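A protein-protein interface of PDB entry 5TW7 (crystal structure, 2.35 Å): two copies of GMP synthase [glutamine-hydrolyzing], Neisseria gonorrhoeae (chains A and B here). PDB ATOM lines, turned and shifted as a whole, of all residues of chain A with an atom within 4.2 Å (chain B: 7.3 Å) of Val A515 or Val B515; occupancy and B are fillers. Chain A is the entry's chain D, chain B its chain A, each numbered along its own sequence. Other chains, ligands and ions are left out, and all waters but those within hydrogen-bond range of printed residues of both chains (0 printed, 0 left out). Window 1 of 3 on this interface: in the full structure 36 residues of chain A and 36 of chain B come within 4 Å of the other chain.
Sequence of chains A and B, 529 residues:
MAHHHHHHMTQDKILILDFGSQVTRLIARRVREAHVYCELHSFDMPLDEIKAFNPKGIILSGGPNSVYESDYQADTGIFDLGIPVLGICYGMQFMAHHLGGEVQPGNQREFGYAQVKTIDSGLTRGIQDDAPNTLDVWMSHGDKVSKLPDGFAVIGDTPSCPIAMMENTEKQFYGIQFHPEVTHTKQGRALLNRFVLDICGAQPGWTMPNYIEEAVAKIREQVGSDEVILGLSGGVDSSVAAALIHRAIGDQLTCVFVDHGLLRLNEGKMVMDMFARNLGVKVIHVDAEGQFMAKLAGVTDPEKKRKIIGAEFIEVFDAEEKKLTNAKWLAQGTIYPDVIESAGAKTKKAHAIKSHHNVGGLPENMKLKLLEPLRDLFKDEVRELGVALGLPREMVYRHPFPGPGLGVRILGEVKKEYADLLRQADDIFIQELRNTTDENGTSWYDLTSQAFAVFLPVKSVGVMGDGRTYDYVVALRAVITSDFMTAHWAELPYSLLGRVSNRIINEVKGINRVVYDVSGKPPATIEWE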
ATOM      1  N   VAL A 474      -2.280   5.144 -14.729  1.00  0.00           N
ATOM      2  CA  VAL A 474      -1.236   6.048 -15.199  1.00  0.00           C
ATOM      3  C   VAL A 474       0.098   5.313 -15.169  1.00  0.00           C
ATOM      4  O   VAL A 474       0.395   4.575 -14.221  1.00  0.00           O
ATOM      5  CB  VAL A 474      -1.208   7.332 -14.346  1.00  0.00           C
ATOM      6  CG1 VAL A 474       0.139   8.006 -14.421  1.00  0.00           C
ATOM      7  CG2 VAL A 474      -2.317   8.285 -14.815  1.00  0.00           C
ATOM      8  N   ALA A 475       0.874   5.476 -16.232  1.00  0.00           N
ATOM      9  CA  ALA A 475       2.240   4.975 -16.300  1.00  0.00           C
ATOM     10  C   ALA A 475       3.225   6.128 -16.163  1.00  0.00           C
ATOM     11  O   ALA A 475       3.052   7.189 -16.787  1.00  0.00           O
ATOM     12  CB  ALA A 475       2.504   4.229 -17.610  1.00  0.00           C
ATOM     13  N   LEU A 476       4.242   5.921 -15.336  1.00  0.00           N
ATOM     14  CA  LEU A 476       5.346   6.860 -15.229  1.00  0.00           C
ATOM     15  C   LEU A 476       6.437   6.405 -16.176  1.00  0.00           C
ATOM     16  O   LEU A 476       6.734   5.212 -16.265  1.00  0.00           O
ATOM     17  CB  LEU A 476       5.880   6.924 -13.795  1.00  0.00           C
ATOM     18  CG  LEU A 476       4.791   7.152 -12.744  1.00  0.00           C
ATOM     19  CD1 LEU A 476       5.356   7.107 -11.342  1.00  0.00           C
ATOM     20  CD2 LEU A 476       4.145   8.499 -13.018  1.00  0.00           C
ATOM     21  N   VAL A 514      -0.954   3.253 -10.456  1.00  0.00           N
ATOM     22  CA  VAL A 514       0.239   3.847 -11.041  1.00  0.00           C
ATOM     23  C   VAL A 514       1.259   2.748 -11.307  1.00  0.00           C
ATOM     24  O   VAL A 514       1.505   1.889 -10.446  1.00  0.00           O
ATOM     25  CB  VAL A 514       0.838   4.943 -10.144  1.00  0.00           C
ATOM     26  CG1 VAL A 514       2.113   5.482 -10.791  1.00  0.00           C
ATOM     27  CG2 VAL A 514      -0.197   6.046  -9.921  1.00  0.00           C
ATOM     28  N   VAL A 515       1.805   2.745 -12.521  1.00  0.00           N
ATOM     29  CA  VAL A 515       2.840   1.806 -12.921  1.00  0.00           C
ATOM     30  C   VAL A 515       4.045   2.609 -13.395  1.00  0.00           C
ATOM     31  O   VAL A 515       3.946   3.802 -13.711  1.00  0.00           O
ATOM     32  CB  VAL A 515       2.347   0.819 -14.008  1.00  0.00           C
ATOM     33  CG1 VAL A 515       1.168   0.021 -13.487  1.00  0.00           C
ATOM     34  CG2 VAL A 515       1.911   1.561 -15.252  1.00  0.00           C
ATOM     35  N   TYR A 516       5.200   1.946 -13.398  1.00  0.00           N
ATOM     36  CA  TYR A 516       6.447   2.533 -13.866  1.00  0.00           C
ATOM     37  C   TYR A 516       6.943   1.739 -15.070  1.00  0.00           C
ATOM     38  O   TYR A 516       7.098   0.516 -14.992  1.00  0.00           O
ATOM     39  CB  TYR A 516       7.514   2.535 -12.766  1.00  0.00           C
ATOM     40  CG  TYR A 516       8.787   3.210 -13.195  1.00  0.00           C
ATOM     41  CD1 TYR A 516       8.754   4.473 -13.769  1.00  0.00           C
ATOM     42  CD2 TYR A 516      10.019   2.590 -13.039  1.00  0.00           C
ATOM     43  CE1 TYR A 516       9.923   5.117 -14.182  1.00  0.00           C
ATOM     44  CE2 TYR A 516      11.190   3.211 -13.448  1.00  0.00           C
ATOM     45  CZ  TYR A 516      11.130   4.489 -14.023  1.00  0.00           C
ATOM     46  OH  TYR A 516      12.272   5.139 -14.432  1.00  0.00           O
ATOM     47  N   ASP A 517       7.230   2.441 -16.159  1.00  0.00           N
ATOM     48  CA  ASP A 517       7.719   1.796 -17.371  1.00  0.00           C
ATOM     49  C   ASP A 517       9.141   1.295 -17.135  1.00  0.00           C
ATOM     50  O   ASP A 517      10.018   2.074 -16.749  1.00  0.00           O
ATOM     51  CB  ASP A 517       7.654   2.797 -18.526  1.00  0.00           C
ATOM     52  CG  ASP A 517       7.935   2.174 -19.889  1.00  0.00           C
ATOM     53  OD1 ASP A 517       8.539   1.089 -19.967  1.00  0.00           O
ATOM     54  OD2 ASP A 517       7.564   2.809 -20.899  1.00  0.00           O
ATOM     55  N   TRP A 528       5.236   6.277 -25.850  1.00  0.00           N
ATOM     56  CA  TRP A 528       4.430   5.086 -26.086  1.00  0.00           C
ATOM     57  C   TRP A 528       3.729   5.102 -27.436  1.00  0.00           C
ATOM     58  O   TRP A 528       3.363   4.036 -27.940  1.00  0.00           O
ATOM     59  CB  TRP A 528       3.384   4.922 -24.991  1.00  0.00           C
ATOM     60  CG  TRP A 528       3.925   4.410 -23.686  1.00  0.00           C
ATOM     61  CD1 TRP A 528       5.098   4.758 -23.091  1.00  0.00           C
ATOM     62  CD2 TRP A 528       3.282   3.493 -22.798  1.00  0.00           C
ATOM     63  NE1 TRP A 528       5.239   4.102 -21.892  1.00  0.00           N
ATOM     64  CE2 TRP A 528       4.136   3.314 -21.690  1.00  0.00           C
ATOM     65  CE3 TRP A 528       2.072   2.794 -22.835  1.00  0.00           C
ATOM     66  CZ2 TRP A 528       3.817   2.465 -20.632  1.00  0.00           C
ATOM     67  CZ3 TRP A 528       1.753   1.943 -21.772  1.00  0.00           C
ATOM     68  CH2 TRP A 528       2.621   1.791 -20.689  1.00  0.00           C
ATOM     69  N   VAL B 454       0.158  -9.114 -15.673  1.00  0.00           N
ATOM     70  CA  VAL B 454      -1.180  -8.647 -16.003  1.00  0.00           C
ATOM     71  C   VAL B 454      -1.183  -8.212 -17.462  1.00  0.00           C
ATOM     72  O   VAL B 454      -0.291  -7.467 -17.891  1.00  0.00           O
ATOM     73  CB  VAL B 454      -1.614  -7.489 -15.081  1.00  0.00           C
ATOM     74  CG1 VAL B 454      -2.930  -6.926 -15.529  1.00  0.00           C
ATOM     75  CG2 VAL B 454      -1.725  -7.969 -13.621  1.00  0.00           C
ATOM     76  N   LEU B 456      -2.568  -6.029 -20.432  1.00  0.00           N
ATOM     77  CA  LEU B 456      -3.288  -4.778 -20.662  1.00  0.00           C
ATOM     78  C   LEU B 456      -3.693  -4.714 -22.120  1.00  0.00           C
ATOM     79  O   LEU B 456      -2.814  -4.780 -22.991  1.00  0.00           O
ATOM     80  CB  LEU B 456      -2.418  -3.571 -20.303  1.00  0.00           C
ATOM     81  CG  LEU B 456      -2.288  -3.084 -18.855  1.00  0.00           C
ATOM     82  CD1 LEU B 456      -2.065  -4.216 -17.894  1.00  0.00           C
ATOM     83  CD2 LEU B 456      -1.172  -2.084 -18.721  1.00  0.00           C
ATOM     84  N   VAL B 473       0.702  -4.407 -23.937  1.00  0.00           N
ATOM     85  CA  VAL B 473       1.490  -4.037 -22.772  1.00  0.00           C
ATOM     86  C   VAL B 473       1.231  -5.047 -21.662  1.00  0.00           C
ATOM     87  O   VAL B 473       0.083  -5.444 -21.438  1.00  0.00           O
ATOM     88  CB  VAL B 473       1.118  -2.613 -22.311  1.00  0.00           C
ATOM     89  CG1 VAL B 473       1.946  -2.193 -21.096  1.00  0.00           C
ATOM     90  CG2 VAL B 473       1.217  -1.627 -23.477  1.00  0.00           C
ATOM     91  N   VAL B 474       2.299  -5.457 -20.972  1.00  0.00           N
ATOM     92  CA  VAL B 474       2.239  -6.345 -19.813  1.00  0.00           C
ATOM     93  C   VAL B 474       2.673  -5.564 -18.572  1.00  0.00           C
ATOM     94  O   VAL B 474       3.642  -4.789 -18.618  1.00  0.00           O
ATOM     95  CB  VAL B 474       3.121  -7.600 -20.034  1.00  0.00           C
ATOM     96  CG1 VAL B 474       3.570  -8.225 -18.712  1.00  0.00           C
ATOM     97  CG2 VAL B 474       2.357  -8.647 -20.862  1.00  0.00           C
ATOM     98  N   ALA B 475       1.932  -5.738 -17.474  1.00  0.00           N
ATOM     99  CA  ALA B 475       2.293  -5.183 -16.171  1.00  0.00           C
ATOM    100  C   ALA B 475       2.800  -6.286 -15.249  1.00  0.00           C
ATOM    101  O   ALA B 475       2.168  -7.344 -15.127  1.00  0.00           O
ATOM    102  CB  ALA B 475       1.103  -4.470 -15.515  1.00  0.00           C
ATOM    103  N   LEU B 476       3.922  -6.033 -14.577  1.00  0.00           N
ATOM    104  CA  LEU B 476       4.424  -6.945 -13.556  1.00  0.00           C
ATOM    105  C   LEU B 476       3.937  -6.487 -12.188  1.00  0.00           C
ATOM    106  O   LEU B 476       4.012  -5.305 -11.854  1.00  0.00           O
ATOM    107  CB  LEU B 476       5.946  -7.023 -13.572  1.00  0.00           C
ATOM    108  CG  LEU B 476       6.578  -7.279 -14.939  1.00  0.00           C
ATOM    109  CD1 LEU B 476       8.076  -7.252 -14.797  1.00  0.00           C
ATOM    110  CD2 LEU B 476       6.113  -8.592 -15.563  1.00  0.00           C
ATOM    111  N   ARG B 477       3.441  -7.429 -11.406  1.00  0.00           N
ATOM    112  CA  ARG B 477       2.906  -7.169 -10.084  1.00  0.00           C
ATOM    113  C   ARG B 477       3.605  -8.102  -9.101  1.00  0.00           C
ATOM    114  O   ARG B 477       3.674  -9.317  -9.327  1.00  0.00           O
ATOM    115  CB  ARG B 477       1.382  -7.364 -10.088  1.00  0.00           C
ATOM    116  CG  ARG B 477       0.681  -7.225  -8.753  1.00  0.00           C
ATOM    117  CD  ARG B 477       1.090  -5.996  -8.073  1.00  0.00           C
ATOM    118  NE  ARG B 477       0.001  -5.370  -7.344  1.00  0.00           N
ATOM    119  CZ  ARG B 477       0.150  -4.216  -6.705  1.00  0.00           C
ATOM    120  NH1 ARG B 477       1.328  -3.618  -6.706  1.00  0.00           N
ATOM    121  NH2 ARG B 477      -0.863  -3.650  -6.084  1.00  0.00           N
ATOM    122  N   LEU B 497      14.167  -6.371 -12.782  1.00  0.00           N
ATOM    123  CA  LEU B 497      13.120  -5.747 -13.593  1.00  0.00           C
ATOM    124  C   LEU B 497      13.572  -5.563 -15.037  1.00  0.00           C
ATOM    125  O   LEU B 497      12.832  -5.893 -15.975  1.00  0.00           O
ATOM    126  CB  LEU B 497      12.707  -4.401 -12.977  1.00  0.00           C
ATOM    127  CG  LEU B 497      11.994  -4.496 -11.619  1.00  0.00           C
ATOM    128  CD1 LEU B 497      11.988  -3.191 -10.827  1.00  0.00           C
ATOM    129  CD2 LEU B 497      10.578  -4.944 -11.854  1.00  0.00           C
ATOM    130  N   SER B 501      11.915  -7.374 -18.323  1.00  0.00           N
ATOM    131  CA  SER B 501      11.425  -6.513 -19.394  1.00  0.00           C
ATOM    132  C   SER B 501      12.028  -6.898 -20.745  1.00  0.00           C
ATOM    133  O   SER B 501      11.305  -7.093 -21.733  1.00  0.00           O
ATOM    134  CB  SER B 501      11.757  -5.064 -19.038  1.00  0.00           C
ATOM    135  OG  SER B 501      11.258  -4.174 -19.988  1.00  0.00           O
ATOM    136  N   ARG B 513       5.919  -3.923 -24.546  1.00  0.00           N
ATOM    137  CA  ARG B 513       6.113  -2.949 -23.484  1.00  0.00           C
ATOM    138  C   ARG B 513       5.783  -3.603 -22.148  1.00  0.00           C
ATOM    139  O   ARG B 513       4.776  -4.313 -22.021  1.00  0.00           O
ATOM    140  CB  ARG B 513       5.249  -1.707 -23.752  1.00  0.00           C
ATOM    141  CG  ARG B 513       5.186  -0.693 -22.626  1.00  0.00           C
ATOM    142  CD  ARG B 513       6.108   0.469 -22.826  1.00  0.00           C
ATOM    143  NE  ARG B 513       6.158   0.950 -24.202  1.00  0.00           N
ATOM    144  CZ  ARG B 513       6.989   1.913 -24.602  1.00  0.00           C
ATOM    145  NH1 ARG B 513       7.814   2.476 -23.721  1.00  0.00           N
ATOM    146  NH2 ARG B 513       7.014   2.307 -25.873  1.00  0.00           N
ATOM    147  N   VAL B 514       6.645  -3.357 -21.156  1.00  0.00           N
ATOM    148  CA  VAL B 514       6.517  -3.942 -19.826  1.00  0.00           C
ATOM    149  C   VAL B 514       6.577  -2.840 -18.783  1.00  0.00           C
ATOM    150  O   VAL B 514       7.520  -2.036 -18.774  1.00  0.00           O
ATOM    151  CB  VAL B 514       7.627  -4.972 -19.551  1.00  0.00           C
ATOM    152  CG1 VAL B 514       7.495  -5.516 -18.116  1.00  0.00           C
ATOM    153  CG2 VAL B 514       7.557  -6.085 -20.555  1.00  0.00           C
ATOM    154  N   VAL B 515       5.599  -2.828 -17.877  1.00  0.00           N
ATOM    155  CA  VAL B 515       5.597  -1.879 -16.771  1.00  0.00           C
ATOM    156  C   VAL B 515       5.559  -2.655 -15.463  1.00  0.00           C
ATOM    157  O   VAL B 515       5.226  -3.839 -15.422  1.00  0.00           O
ATOM    158  CB  VAL B 515       4.424  -0.882 -16.830  1.00  0.00           C
ATOM    159  CG1 VAL B 515       4.444  -0.124 -18.162  1.00  0.00           C
ATOM    160  CG2 VAL B 515       3.087  -1.596 -16.575  1.00  0.00           C
ATOM    161  N   TYR B 516       5.940  -1.973 -14.386  1.00  0.00           N
ATOM    162  CA  TYR B 516       5.902  -2.544 -13.050  1.00  0.00           C
ATOM    163  C   TYR B 516       4.946  -1.728 -12.184  1.00  0.00           C
ATOM    164  O   TYR B 516       5.057  -0.498 -12.097  1.00  0.00           O
ATOM    165  CB  TYR B 516       7.305  -2.592 -12.438  1.00  0.00           C
ATOM    166  CG  TYR B 516       7.345  -3.234 -11.089  1.00  0.00           C
ATOM    167  CD1 TYR B 516       6.736  -4.467 -10.870  1.00  0.00           C
ATOM    168  CD2 TYR B 516       7.984  -2.615 -10.017  1.00  0.00           C
ATOM    169  CE1 TYR B 516       6.768  -5.084  -9.603  1.00  0.00           C
ATOM    170  CE2 TYR B 516       8.023  -3.225  -8.756  1.00  0.00           C
ATOM    171  CZ  TYR B 516       7.412  -4.460  -8.563  1.00  0.00           C
ATOM    172  OH  TYR B 516       7.440  -5.062  -7.320  1.00  0.00           O
ATOM    173  N   ASP B 517       4.019  -2.424 -11.543  1.00  0.00           N
ATOM    174  CA  ASP B 517       3.021  -1.805 -10.686  1.00  0.00           C
ATOM    175  C   ASP B 517       3.694  -1.284  -9.422  1.00  0.00           C
ATOM    176  O   ASP B 517       4.294  -2.059  -8.672  1.00  0.00           O
ATOM    177  CB  ASP B 517       1.946  -2.844 -10.355  1.00  0.00           C
ATOM    178  CG  ASP B 517       0.750  -2.266  -9.615  1.00  0.00           C
ATOM    179  OD1 ASP B 517       0.866  -1.173  -9.008  1.00  0.00           O
ATOM    180  OD2 ASP B 517      -0.310  -2.933  -9.638  1.00  0.00           O
ATOM    181  N   VAL B 518       3.586   0.020  -9.174  1.00  0.00           N
ATOM    182  CA  VAL B 518       4.208   0.598  -7.984  1.00  0.00           C
ATOM    183  C   VAL B 518       3.143   1.148  -7.038  1.00  0.00           C
ATOM    184  O   VAL B 518       3.390   2.094  -6.285  1.00  0.00           O
ATOM    185  CB  VAL B 518       5.237   1.689  -8.352  1.00  0.00           C
ATOM    186  CG1 VAL B 518       6.468   1.047  -9.013  1.00  0.00           C
ATOM    187  CG2 VAL B 518       4.603   2.830  -9.205  1.00  0.00           C
ATOM    188  N   SER B 519       1.976   0.519  -7.040  1.00  0.00           N
ATOM    189  CA  SER B 519       0.862   0.885  -6.173  1.00  0.00           C
ATOM    190  C   SER B 519       0.797  -0.111  -5.023  1.00  0.00           C
ATOM    191  O   SER B 519       0.758  -1.323  -5.250  1.00  0.00           O
ATOM    192  CB  SER B 519      -0.460   0.880  -6.942  1.00  0.00           C
ATOM    193  OG  SER B 519      -0.398   1.654  -8.126  1.00  0.00           O
ATOM    194  N   TRP B 528      -5.618  -6.604 -10.162  1.00  0.00           N
ATOM    195  CA  TRP B 528      -6.107  -5.446 -10.897  1.00  0.00           C
ATOM    196  C   TRP B 528      -7.614  -5.472 -11.097  1.00  0.00           C
ATOM    197  O   TRP B 528      -8.213  -4.424 -11.345  1.00  0.00           O
ATOM    198  CB  TRP B 528      -5.401  -5.342 -12.256  1.00  0.00           C
ATOM    199  CG  TRP B 528      -3.991  -4.760 -12.187  1.00  0.00           C
ATOM    200  CD1 TRP B 528      -3.028  -5.031 -11.256  1.00  0.00           C
ATOM    201  CD2 TRP B 528      -3.418  -3.792 -13.083  1.00  0.00           C
ATOM    202  NE1 TRP B 528      -1.885  -4.298 -11.526  1.00  0.00           N
ATOM    203  CE2 TRP B 528      -2.101  -3.530 -12.637  1.00  0.00           C
ATOM    204  CE3 TRP B 528      -3.896  -3.117 -14.208  1.00  0.00           C
ATOM    205  CZ2 TRP B 528      -1.255  -2.611 -13.277  1.00  0.00           C
ATOM    206  CZ3 TRP B 528      -3.050  -2.204 -14.851  1.00  0.00           C
ATOM    207  CH2 TRP B 528      -1.742  -1.969 -14.383  1.00  0.00           C
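NH1 of Arg B513 is in salt-bridge range of OD2 of Asp A517 (2.9 Å).
N of Tyr A516 is in hydrogen-bond range of O of Tyr B516.
N of Val B518 sits at hydrogen-bond distance from O of Val A514 (3.1 Å).
OG of Ser B519 sits at hydrogen-bond distance from N of Val A514.
OD1 of Asp B517 sits close to O of Val A514 (3.4 Å).
OD1 of Asp A517 sits close to O of Val B514, at 3.5 Å.
Val A514 touches Asp B517, and with the chains exchanged Asp A517 touches Val B514.
Val A515 touches Tyr B516, and with the chains exchanged Tyr A516 touches Val B515.
Val A515 touches Asp B517, and with the chains exchanged Asp A517 touches Val B515.
Tyr B516 touches its own counterpart, Tyr A516.
Val A515 touches four residues of chain B.
Of the printed residues of chain B, Asp A517 touches Arg B513 (2.9 Å), Val B514 (3.5 Å) and Val B515 (3.9 Å).
Of the printed residues of chain A, Val B473 touches Trp A528.
Printed residues of chain A within 4 Å of Val B514: Asp A517.
Val B515 touches four residues of chain A.
Of the printed residues of chain A, Tyr B516 touches Val A515 (3.3 Å) and Tyr A516 (2.8 Å).
Printed residues of chain A within 4 Å of Ser B519: Val A514.
The nearest printed residue of chain A that does not touch Tyr B516 is Val A514 (4.6 Å).
The backbone NH (N) of Leu B456 lies within hydrogen-bond range of the backbone carbonyl oxygen (O) of Val B473 (2.9 Å).
The backbone NH (N) of Val B474 is in hydrogen-bond range of the backbone carbonyl oxygen (O) of Arg B513, at 2.9 Å.
The backbone carbonyl oxygen (O) of Val A474 lies within hydrogen-bond range of the backbone NH (N) of Val A515, 2.9 Å away.
N of Leu A476 is in hydrogen-bond range of O of Val A515 (2.7 Å).
The backbone carbonyl oxygen (O) of Leu A476 sits at hydrogen-bond distance from the backbone NH (N) of Asp A517 (2.8 Å).
OD2 of Asp A517 sits at hydrogen-bond distance from NE1 of Trp A528.
Val A515 touches Val B515 (CB to CG2, 3.6 Å).
Val A515 touches Tyr B516.
Val A515 touches Asp B517 (CG1 to CA, 3.8 Å).
Val A515 touches Trp B528.
Tyr A516 touches Val B515 (O to CA, 3.3 Å).
CA of Asp A517 touches CG1 of Val B515, at 3.9 Å.
Val B473 touches Trp A528.
Arg B513 touches Trp A528 (NH1 to NE1, 3.6 Å).
CG1 of Val B515 touches CZ2 of Trp A528, at 3.6 Å.
Hydrophobic or aromatic side chains of chain B that line the printed part of chain A: Val B473, Val B515, Val B518 and Trp B528.
Along chain B the printed residues that touch a printed residue of chain A span positions 473 to 528.
Of the 8 printed residues of chain A, 5 touch a printed residue of chain B.
Among the printed residues, 15 pairs touch across the chains.
Among the printed residues, Asp or Glu carboxylates within 4 Å of a Lys or Arg side-chain nitrogen of the other chain: Asp A517 with Arg B513 (2.9 Å).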
